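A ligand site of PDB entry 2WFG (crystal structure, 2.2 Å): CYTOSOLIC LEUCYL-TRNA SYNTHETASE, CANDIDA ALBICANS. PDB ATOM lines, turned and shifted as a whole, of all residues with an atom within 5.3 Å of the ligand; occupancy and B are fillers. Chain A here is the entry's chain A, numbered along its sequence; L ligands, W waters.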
ATOM      1  N   TYR A   3      -5.191  -2.327 -15.781  1.00  0.00           N
ATOM      2  CA  TYR A   3      -5.027  -2.652 -17.207  1.00  0.00           C
ATOM      3  C   TYR A   3      -4.479  -1.471 -17.968  1.00  0.00           C
ATOM      4  O   TYR A   3      -4.614  -0.315 -17.534  1.00  0.00           O
ATOM      5  CB  TYR A   3      -6.369  -3.044 -17.827  1.00  0.00           C
ATOM      6  CG  TYR A   3      -6.873  -4.423 -17.496  1.00  0.00           C
ATOM      7  CD1 TYR A   3      -6.254  -5.553 -18.030  1.00  0.00           C
ATOM      8  CD2 TYR A   3      -7.980  -4.609 -16.675  1.00  0.00           C
ATOM      9  CE1 TYR A   3      -6.713  -6.831 -17.737  1.00  0.00           C
ATOM     10  CE2 TYR A   3      -8.452  -5.887 -16.383  1.00  0.00           C
ATOM     11  CZ  TYR A   3      -7.819  -6.988 -16.913  1.00  0.00           C
ATOM     12  OH  TYR A   3      -8.269  -8.256 -16.625  1.00  0.00           O
ATOM     13  N   ALA A  38      -8.139  -3.997 -23.729  1.00  0.00           N
ATOM     14  CA  ALA A  38      -7.521  -4.061 -22.406  1.00  0.00           C
ATOM     15  C   ALA A  38      -6.388  -5.063 -22.449  1.00  0.00           C
ATOM     16  O   ALA A  38      -6.607  -6.231 -22.783  1.00  0.00           O
ATOM     17  CB  ALA A  38      -8.553  -4.470 -21.350  1.00  0.00           C
ATOM     18  N   THR A  39      -5.177  -4.589 -22.152  1.00  0.00           N
ATOM     19  CA  THR A  39      -3.981  -5.440 -22.112  1.00  0.00           C
ATOM     20  C   THR A  39      -3.140  -5.299 -20.840  1.00  0.00           C
ATOM     21  O   THR A  39      -3.168  -4.259 -20.145  1.00  0.00           O
ATOM     22  CB  THR A  39      -3.058  -5.215 -23.309  1.00  0.00           C
ATOM     23  OG1 THR A  39      -2.077  -6.271 -23.352  1.00  0.00           O
ATOM     24  CG2 THR A  39      -2.337  -3.839 -23.222  1.00  0.00           C
ATOM     25  N   LEU A  40      -2.389  -6.361 -20.547  1.00  0.00           N
ATOM     26  CA  LEU A  40      -1.364  -6.349 -19.514  1.00  0.00           C
ATOM     27  C   LEU A  40       0.021  -6.422 -20.150  1.00  0.00           C
ATOM     28  O   LEU A  40       1.050  -6.543 -19.469  1.00  0.00           O
ATOM     29  CB  LEU A  40      -1.571  -7.531 -18.562  1.00  0.00           C
ATOM     30  CG  LEU A  40      -2.702  -7.361 -17.539  1.00  0.00           C
ATOM     31  CD1 LEU A  40      -2.800  -8.594 -16.629  1.00  0.00           C
ATOM     32  CD2 LEU A  40      -2.495  -6.113 -16.686  1.00  0.00           C
ATOM     33  N   ARG A  41       0.046  -6.356 -21.485  1.00  0.00           N
ATOM     34  CA  ARG A  41       1.306  -6.547 -22.202  1.00  0.00           C
ATOM     35  C   ARG A  41       1.510  -5.502 -23.321  1.00  0.00           C
ATOM     36  O   ARG A  41       1.579  -5.863 -24.496  1.00  0.00           O
ATOM     37  CB  ARG A  41       1.434  -7.998 -22.717  1.00  0.00           C
ATOM     38  CG  ARG A  41       1.666  -9.032 -21.597  1.00  0.00           C
ATOM     39  CD  ARG A  41       2.210 -10.359 -22.132  1.00  0.00           C
ATOM     40  NE  ARG A  41       3.625 -10.282 -22.519  1.00  0.00           N
ATOM     41  CZ  ARG A  41       4.351 -11.325 -22.948  1.00  0.00           C
ATOM     42  NH1 ARG A  41       3.797 -12.527 -23.045  1.00  0.00           N
ATOM     43  NH2 ARG A  41       5.627 -11.177 -23.267  1.00  0.00           N
ATOM     44  N   THR A  44       3.911  -5.952 -26.338  1.00  0.00           N
ATOM     45  CA  THR A  44       3.602  -6.863 -27.456  1.00  0.00           C
ATOM     46  C   THR A  44       2.887  -6.174 -28.629  1.00  0.00           C
ATOM     47  O   THR A  44       2.701  -6.794 -29.682  1.00  0.00           O
ATOM     48  CB  THR A  44       2.758  -8.076 -27.002  1.00  0.00           C
ATOM     49  OG1 THR A  44       1.492  -7.618 -26.479  1.00  0.00           O
ATOM     50  CG2 THR A  44       3.494  -8.887 -25.949  1.00  0.00           C
ATOM     51  N   MET A  45       2.525  -4.896 -28.461  1.00  0.00           N
ATOM     52  CA  MET A  45       1.689  -4.177 -29.433  1.00  0.00           C
ATOM     53  C   MET A  45       2.259  -4.191 -30.838  1.00  0.00           C
ATOM     54  O   MET A  45       1.492  -4.141 -31.787  1.00  0.00           O
ATOM     55  CB  MET A  45       1.390  -2.733 -28.988  1.00  0.00           C
ATOM     56  CG  MET A  45       0.476  -2.600 -27.757  1.00  0.00           C
ATOM     57  SD  MET A  45      -1.130  -3.454 -27.836  1.00  0.00           S
ATOM     58  CE  MET A  45      -0.714  -5.048 -27.107  1.00  0.00           C
ATOM     59  N   THR A 125     -14.501 -16.534 -26.962  1.00  0.00           N
ATOM     60  CA  THR A 125     -14.078 -16.813 -25.599  1.00  0.00           C
ATOM     61  C   THR A 125     -13.729 -15.548 -24.792  1.00  0.00           C
ATOM     62  O   THR A 125     -13.011 -15.611 -23.793  1.00  0.00           O
ATOM     63  CB  THR A 125     -12.890 -17.815 -25.557  1.00  0.00           C
ATOM     64  OG1 THR A 125     -11.802 -17.283 -26.297  1.00  0.00           O
ATOM     65  CG2 THR A 125     -13.303 -19.164 -26.155  1.00  0.00           C
ATOM     66  N   VAL A 126     -14.243 -14.395 -25.237  1.00  0.00           N
ATOM     67  CA  VAL A 126     -14.089 -13.146 -24.483  1.00  0.00           C
ATOM     68  C   VAL A 126     -14.974 -13.226 -23.236  1.00  0.00           C
ATOM     69  O   VAL A 126     -16.121 -13.620 -23.306  1.00  0.00           O
ATOM     70  CB  VAL A 126     -14.438 -11.878 -25.328  1.00  0.00           C
ATOM     71  CG1 VAL A 126     -14.526 -10.629 -24.446  1.00  0.00           C
ATOM     72  CG2 VAL A 126     -13.417 -11.664 -26.450  1.00  0.00           C
ATOM     73  N   LEU A 127     -14.378 -12.883 -22.092  1.00  0.00           N
ATOM     74  CA  LEU A 127     -15.121 -12.819 -20.838  1.00  0.00           C
ATOM     75  C   LEU A 127     -15.724 -11.427 -20.697  1.00  0.00           C
ATOM     76  O   LEU A 127     -14.992 -10.426 -20.573  1.00  0.00           O
ATOM     77  CB  LEU A 127     -14.204 -13.186 -19.660  1.00  0.00           C
ATOM     78  CG  LEU A 127     -14.844 -13.168 -18.262  1.00  0.00           C
ATOM     79  CD1 LEU A 127     -16.143 -13.988 -18.196  1.00  0.00           C
ATOM     80  CD2 LEU A 127     -13.854 -13.648 -17.220  1.00  0.00           C
ATOM     81  N   ALA A 128     -17.055 -11.373 -20.747  1.00  0.00           N
ATOM     82  CA  ALA A 128     -17.809 -10.115 -20.848  1.00  0.00           C
ATOM     83  C   ALA A 128     -17.587  -9.197 -19.647  1.00  0.00           C
ATOM     84  O   ALA A 128     -17.616  -7.958 -19.801  1.00  0.00           O
ATOM     85  CB  ALA A 128     -19.309 -10.405 -21.022  1.00  0.00           C
ATOM     86  N   LYS A 130     -14.793  -8.934 -17.875  1.00  0.00           N
ATOM     87  CA  LYS A 130     -13.366  -8.643 -17.681  1.00  0.00           C
ATOM     88  C   LYS A 130     -12.862  -7.591 -18.679  1.00  0.00           C
ATOM     89  O   LYS A 130     -13.167  -7.653 -19.868  1.00  0.00           O
ATOM     90  CB  LYS A 130     -12.543  -9.933 -17.832  1.00  0.00           C
ATOM     91  CG  LYS A 130     -11.046  -9.776 -17.632  1.00  0.00           C
ATOM     92  CD  LYS A 130     -10.331 -10.975 -18.238  1.00  0.00           C
ATOM     93  CE  LYS A 130      -9.138 -11.437 -17.406  1.00  0.00           C
ATOM     94  NZ  LYS A 130      -8.896 -12.894 -17.665  1.00  0.00           N
ATOM     95  N   GLY A 131     -12.081  -6.632 -18.188  1.00  0.00           N
ATOM     96  CA  GLY A 131     -11.524  -5.595 -19.038  1.00  0.00           C
ATOM     97  C   GLY A 131     -12.611  -4.833 -19.778  1.00  0.00           C
ATOM     98  O   GLY A 131     -13.663  -4.511 -19.198  1.00  0.00           O
ATOM     99  N   THR A 132     -12.375  -4.590 -21.067  1.00  0.00           N
ATOM    100  CA  THR A 132     -13.296  -3.801 -21.872  1.00  0.00           C
ATOM    101  C   THR A 132     -14.175  -4.653 -22.773  1.00  0.00           C
ATOM    102  O   THR A 132     -15.067  -4.135 -23.466  1.00  0.00           O
ATOM    103  CB  THR A 132     -12.539  -2.812 -22.745  1.00  0.00           C
ATOM    104  OG1 THR A 132     -11.694  -3.551 -23.644  1.00  0.00           O
ATOM    105  CG2 THR A 132     -11.686  -1.884 -21.891  1.00  0.00           C
ATOM    106  N   GLY A 133     -13.918  -5.969 -22.784  1.00  0.00           N
ATOM    107  CA  GLY A 133     -14.578  -6.900 -23.702  1.00  0.00           C
ATOM    108  C   GLY A 133     -13.990  -6.825 -25.098  1.00  0.00           C
ATOM    109  O   GLY A 133     -14.411  -7.556 -26.015  1.00  0.00           O
ATOM    110  N   VAL A 134     -13.019  -5.933 -25.254  1.00  0.00           N
ATOM    111  CA  VAL A 134     -12.251  -5.777 -26.502  1.00  0.00           C
ATOM    112  C   VAL A 134     -10.882  -6.364 -26.223  1.00  0.00           C
ATOM    113  O   VAL A 134     -10.261  -6.073 -25.194  1.00  0.00           O
ATOM    114  CB  VAL A 134     -12.187  -4.286 -26.983  1.00  0.00           C
ATOM    115  CG1 VAL A 134     -11.366  -4.130 -28.261  1.00  0.00           C
ATOM    116  CG2 VAL A 134     -13.592  -3.732 -27.212  1.00  0.00           C
ATOM    117  N   VAL A 135     -10.423  -7.238 -27.113  1.00  0.00           N
ATOM    118  CA  VAL A 135      -9.182  -7.982 -26.918  1.00  0.00           C
ATOM    119  C   VAL A 135      -8.325  -7.911 -28.169  1.00  0.00           C
ATOM    120  O   VAL A 135      -8.760  -8.316 -29.257  1.00  0.00           O
ATOM    121  CB  VAL A 135      -9.434  -9.458 -26.529  1.00  0.00           C
ATOM    122  CG1 VAL A 135      -8.134 -10.244 -26.487  1.00  0.00           C
ATOM    123  CG2 VAL A 135     -10.139  -9.525 -25.167  1.00  0.00           C
ATOM    124  N   THR A 136      -7.135  -7.354 -28.025  1.00  0.00           N
ATOM    125  CA  THR A 136      -6.272  -7.201 -29.170  1.00  0.00           C
ATOM    126  C   THR A 136      -5.427  -8.458 -29.373  1.00  0.00           C
ATOM    127  O   THR A 136      -5.029  -9.116 -28.405  1.00  0.00           O
ATOM    128  CB  THR A 136      -5.458  -5.887 -29.113  1.00  0.00           C
ATOM    129  OG1 THR A 136      -4.741  -5.720 -30.345  1.00  0.00           O
ATOM    130  CG2 THR A 136      -4.471  -5.876 -27.934  1.00  0.00           C
ATOM    131  N   VAL A 138      -2.480 -10.934 -30.479  1.00  0.00           N
ATOM    132  CA  VAL A 138      -1.020 -11.042 -30.589  1.00  0.00           C
ATOM    133  C   VAL A 138      -0.627 -12.543 -30.627  1.00  0.00           C
ATOM    134  O   VAL A 138      -0.281 -13.132 -29.610  1.00  0.00           O
ATOM    135  CB  VAL A 138      -0.316 -10.243 -29.427  1.00  0.00           C
ATOM    136  CG1 VAL A 138       1.199 -10.388 -29.469  1.00  0.00           C
ATOM    137  CG2 VAL A 138      -0.701  -8.746 -29.459  1.00  0.00           C
ATOM    138  N   ASP A 141       2.604 -14.405 -28.885  1.00  0.00           N
ATOM    139  CA  ASP A 141       2.876 -14.442 -27.450  1.00  0.00           C
ATOM    140  C   ASP A 141       1.652 -14.688 -26.568  1.00  0.00           C
ATOM    141  O   ASP A 141       1.771 -14.832 -25.345  1.00  0.00           O
ATOM    142  CB  ASP A 141       3.639 -13.174 -27.038  1.00  0.00           C
ATOM    143  CG  ASP A 141       5.050 -13.154 -27.594  1.00  0.00           C
ATOM    144  OD1 ASP A 141       5.972 -13.652 -26.910  1.00  0.00           O
ATOM    145  OD2 ASP A 141       5.246 -12.670 -28.734  1.00  0.00           O
ATOM    146  N   SER A 142       0.479 -14.746 -27.194  1.00  0.00           N
ATOM    147  CA  SER A 142      -0.737 -15.059 -26.481  1.00  0.00           C
ATOM    148  C   SER A 142      -1.306 -16.416 -26.891  1.00  0.00           C
ATOM    149  O   SER A 142      -1.780 -16.585 -28.023  1.00  0.00           O
ATOM    150  CB  SER A 142      -1.795 -13.989 -26.695  1.00  0.00           C
ATOM    151  OG  SER A 142      -3.074 -14.507 -26.404  1.00  0.00           O
ATOM    152  N   PRO A 143      -1.292 -17.395 -25.964  1.00  0.00           N
ATOM    153  CA  PRO A 143      -1.867 -18.698 -26.299  1.00  0.00           C
ATOM    154  C   PRO A 143      -3.317 -18.611 -26.804  1.00  0.00           C
ATOM    155  O   PRO A 143      -3.637 -19.186 -27.847  1.00  0.00           O
ATOM    156  CB  PRO A 143      -1.765 -19.471 -24.982  1.00  0.00           C
ATOM    157  CG  PRO A 143      -0.554 -18.896 -24.313  1.00  0.00           C
ATOM    158  CD  PRO A 143      -0.570 -17.431 -24.669  1.00  0.00           C
ATOM    159  N   ASP A 145      -4.860 -16.147 -28.240  1.00  0.00           N
ATOM    160  CA  ASP A 145      -4.927 -15.458 -29.531  1.00  0.00           C
ATOM    161  C   ASP A 145      -4.432 -16.356 -30.633  1.00  0.00           C
ATOM    162  O   ASP A 145      -4.952 -16.293 -31.752  1.00  0.00           O
ATOM    163  CB  ASP A 145      -4.117 -14.151 -29.511  1.00  0.00           C
ATOM    164  CG  ASP A 145      -4.654 -13.143 -28.491  1.00  0.00           C
ATOM    165  OD1 ASP A 145      -5.799 -13.320 -28.024  1.00  0.00           O
ATOM    166  OD2 ASP A 145      -3.920 -12.179 -28.156  1.00  0.00           O
ATOM    167  N   LYS A 206      -0.935 -19.722 -20.678  1.00  0.00           N
ATOM    168  CA  LYS A 206      -0.914 -18.258 -20.538  1.00  0.00           C
ATOM    169  C   LYS A 206      -0.001 -17.859 -19.395  1.00  0.00           C
ATOM    170  O   LYS A 206       0.826 -16.961 -19.539  1.00  0.00           O
ATOM    171  CB  LYS A 206      -2.317 -17.723 -20.282  1.00  0.00           C
ATOM    172  CG  LYS A 206      -2.402 -16.220 -20.322  1.00  0.00           C
ATOM    173  CD  LYS A 206      -3.825 -15.774 -20.190  1.00  0.00           C
ATOM    174  CE  LYS A 206      -3.891 -14.268 -20.142  1.00  0.00           C
ATOM    175  NZ  LYS A 206      -5.305 -13.803 -20.015  1.00  0.00           N
ATOM    176  N   ALA A 209       3.630 -18.575 -20.291  1.00  0.00           N
ATOM    177  CA  ALA A 209       4.099 -17.575 -21.254  1.00  0.00           C
ATOM    178  C   ALA A 209       4.361 -16.224 -20.587  1.00  0.00           C
ATOM    179  O   ALA A 209       5.387 -15.607 -20.857  1.00  0.00           O
ATOM    180  CB  ALA A 209       3.134 -17.447 -22.434  1.00  0.00           C
ATOM    181  N   TYR A 210       3.452 -15.801 -19.711  1.00  0.00           N
ATOM    182  CA  TYR A 210       3.625 -14.590 -18.887  1.00  0.00           C
ATOM    183  C   TYR A 210       4.978 -14.506 -18.195  1.00  0.00           C
ATOM    184  O   TYR A 210       5.765 -13.604 -18.486  1.00  0.00           O
ATOM    185  CB  TYR A 210       2.534 -14.505 -17.815  1.00  0.00           C
ATOM    186  CG  TYR A 210       1.327 -13.651 -18.141  1.00  0.00           C
ATOM    187  CD1 TYR A 210       1.467 -12.411 -18.789  1.00  0.00           C
ATOM    188  CD2 TYR A 210       0.050 -14.057 -17.749  1.00  0.00           C
ATOM    189  CE1 TYR A 210       0.337 -11.614 -19.067  1.00  0.00           C
ATOM    190  CE2 TYR A 210      -1.083 -13.281 -18.015  1.00  0.00           C
ATOM    191  CZ  TYR A 210      -0.942 -12.069 -18.679  1.00  0.00           C
ATOM    192  OH  TYR A 210      -2.069 -11.314 -18.939  1.00  0.00           O
HETATM  193  C1  LIG L   1      -2.380  -8.506 -25.489  1.00  0.00           C
HETATM  194  C2  LIG L   1      -1.628  -9.562 -25.145  1.00  0.00           C
HETATM  195  C3  LIG L   1      -0.468 -10.092 -25.707  1.00  0.00           C
HETATM  196  C4  LIG L   1      -2.173 -10.170 -24.012  1.00  0.00           C
HETATM  197  C5  LIG L   1       0.144 -11.208 -25.156  1.00  0.00           C
HETATM  198  C6  LIG L   1      -1.577 -11.297 -23.449  1.00  0.00           C
HETATM  199  C7  LIG L   1      -0.409 -11.817 -24.016  1.00  0.00           C
HETATM  200  P1  LIG L   1      -5.496 -11.688 -17.345  1.00  0.00           P
HETATM  201  O1  LIG L   1      -6.108 -13.165 -17.119  1.00  0.00           O
HETATM  202  O2  LIG L   1      -3.872 -11.827 -17.152  1.00  0.00           O
HETATM  203  O3  LIG L   1      -6.107 -10.636 -16.466  1.00  0.00           O
HETATM  204  N1  LIG L   1      -7.838 -10.108 -22.074  1.00  0.00           N
HETATM  205  C8  LIG L   1      -8.292  -8.913 -21.702  1.00  0.00           C
HETATM  206  N2  LIG L   1      -9.603  -8.967 -21.537  1.00  0.00           N
HETATM  207  C9  LIG L   1      -9.985 -10.215 -21.789  1.00  0.00           C
HETATM  208  C10 LIG L   1     -11.225 -10.842 -21.773  1.00  0.00           C
HETATM  209  N3  LIG L   1     -12.327 -10.155 -21.457  1.00  0.00           N
HETATM  210  N4  LIG L   1     -11.296 -12.140 -22.085  1.00  0.00           N
HETATM  211  C11 LIG L   1     -10.201 -12.827 -22.395  1.00  0.00           C
HETATM  212  N5  LIG L   1      -9.000 -12.258 -22.412  1.00  0.00           N
HETATM  213  C12 LIG L   1      -8.863 -10.962 -22.114  1.00  0.00           C
HETATM  214  O4  LIG L   1      -5.695 -11.324 -18.890  1.00  0.00           O
HETATM  215  C13 LIG L   1      -5.117 -10.129 -19.468  1.00  0.00           C
HETATM  216  C14 LIG L   1      -4.779 -10.440 -20.916  1.00  0.00           C
HETATM  217  O5  LIG L   1      -5.818 -11.308 -21.537  1.00  0.00           O
HETATM  218  C15 LIG L   1      -4.734  -9.168 -21.779  1.00  0.00           C
HETATM  219  O6  LIG L   1      -3.437  -8.915 -22.295  1.00  0.00           O
HETATM  220  C16 LIG L   1      -5.571  -9.524 -23.002  1.00  0.00           C
HETATM  221  O7  LIG L   1      -4.611 -10.186 -23.818  1.00  0.00           O
HETATM  222  C17 LIG L   1      -6.556 -10.421 -22.284  1.00  0.00           C
HETATM  223  F1  LIG L   1       1.271 -11.696 -25.725  1.00  0.00           F
HETATM  224  O8  LIG L   1      -3.448  -8.315 -24.642  1.00  0.00           O
HETATM  225  B1  LIG L   1      -3.436  -9.367 -23.670  1.00  0.00           B
HETATM  226  C18 LIG L   1       0.832 -14.595 -21.874  1.00  0.00           C
HETATM  227  C19 LIG L   1      -0.297 -13.653 -22.342  1.00  0.00           C
HETATM  228  N6  LIG L   1       0.201 -12.900 -23.498  1.00  0.00           N
HETATM  229  O   HOH W   1      -4.840 -10.705 -26.353  1.00  0.00           O
HETATM  230  O   HOH W   2      -2.194 -11.611 -14.793  1.00  0.00           O
HETATM  231  O   HOH W   3     -10.994  -6.677 -22.255  1.00  0.00           O
HETATM  232  O   HOH W   4      -7.167 -14.141 -22.640  1.00  0.00           O
HETATM  233  O   HOH W   5      -5.770  -7.036 -25.366  1.00  0.00           O
HETATM  234  O   HOH W   6      -8.980 -14.845 -24.731  1.00  0.00           O
HETATM  235  O   HOH W   7      -4.113 -13.327 -24.002  1.00  0.00           O
HETATM  236  O   HOH W   8      -5.399  -9.391 -13.857  1.00  0.00           O
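The side-chain hydroxyl of Tyr 210 lies within hydrogen-bond range of an oxygen (O2) of the ligand (2.6 Å).
NZ of Lys 206 is in salt-bridge range of O1 of the ligand (3.1 Å).
The side-chain hydroxyl (OG1) of Thr 39 is in hydrogen-bond range of an oxygen (O8) of the ligand, 2.8 Å away.
N4 of the ligand is in hydrogen-bond range of N of Leu 127 (3.2 Å).
The backbone carbonyl oxygen (O) of Leu 127 sits at hydrogen-bond distance from a nitrogen (N3) of the ligand.
A nitrogen (N3) of the ligand sits at hydrogen-bond distance from the backbone carbonyl oxygen (O) of Lys 130, 3.1 Å away.
O1 of the ligand is in salt-bridge range of NZ of Lys 130, 2.9 Å away.
The backbone carbonyl oxygen (O) of Asp 141 is in hydrogen-bond range of a nitrogen (N6) of the ligand (3.1 Å).
O3 of the ligand lies within hydrogen-bond range of OH of Tyr 3 (3.2 Å).
The backbone NH of Leu 40 is in hydrogen-bond range of an oxygen (O6) of the ligand (3.3 Å).
The side-chain hydroxyl (OG1) of Thr 39 lies within hydrogen-bond range of the backbone NH (N) of Arg 41.
The side-chain hydroxyl (OG1) of Thr 44 sits at hydrogen-bond distance from the backbone carbonyl oxygen (O) of Arg 41 (2.6 Å).
The backbone NH (N) of Ala 38 is in hydrogen-bond range of the backbone carbonyl oxygen (O) of Val 134.
The side-chain hydroxyl (OG) of Ser 142 sits close to the side-chain carboxylate (OD2) of Asp 145 (3.0 Å).
The backbone NH (N) of Val 138 lies within hydrogen-bond range of the side-chain carboxylate (OD2) of Asp 145.
A fluorine (F1) of the ligand lies close to the backbone NH of Ser 142, at 3.5 Å.
O of Ala 38 touches C8 of the ligand, at 3.3 Å.
CD of Arg 41 touches N6 of the ligand, at 3.5 Å.
OG1 of Thr 44 touches C3 of the ligand, 3.2 Å away.
CG1 of Val 126 touches N3 of the ligand, at 3.7 Å.
Val 135 touches the ligand.
Thr 136 touches the ligand (O to C1, 3.99 Å).
Val 138 touches the ligand (CB to C3, 3.7 Å).
CB of Ala 209 touches C18 of the ligand, 3.7 Å away.
Hydrophobic or aromatic side chains within 4 Å of the ligand: Leu 40, Val 126, Leu 127, Val 135, Val 138, Ala 209 and Tyr 210.
Water W4 lies within hydrogen-bond range of N5 of the ligand (2.6 Å) and NZ of Lys 206 (3.2 Å).
Water W5 lies within hydrogen-bond range of O8 of the ligand (2.7 Å), O of Ala 38 (2.8 Å) and N of Thr 136 (3.0 Å).
Water W7 bridges the side-chain hydroxyl (OG) of Ser 142 and an oxygen (O7) of the ligand.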
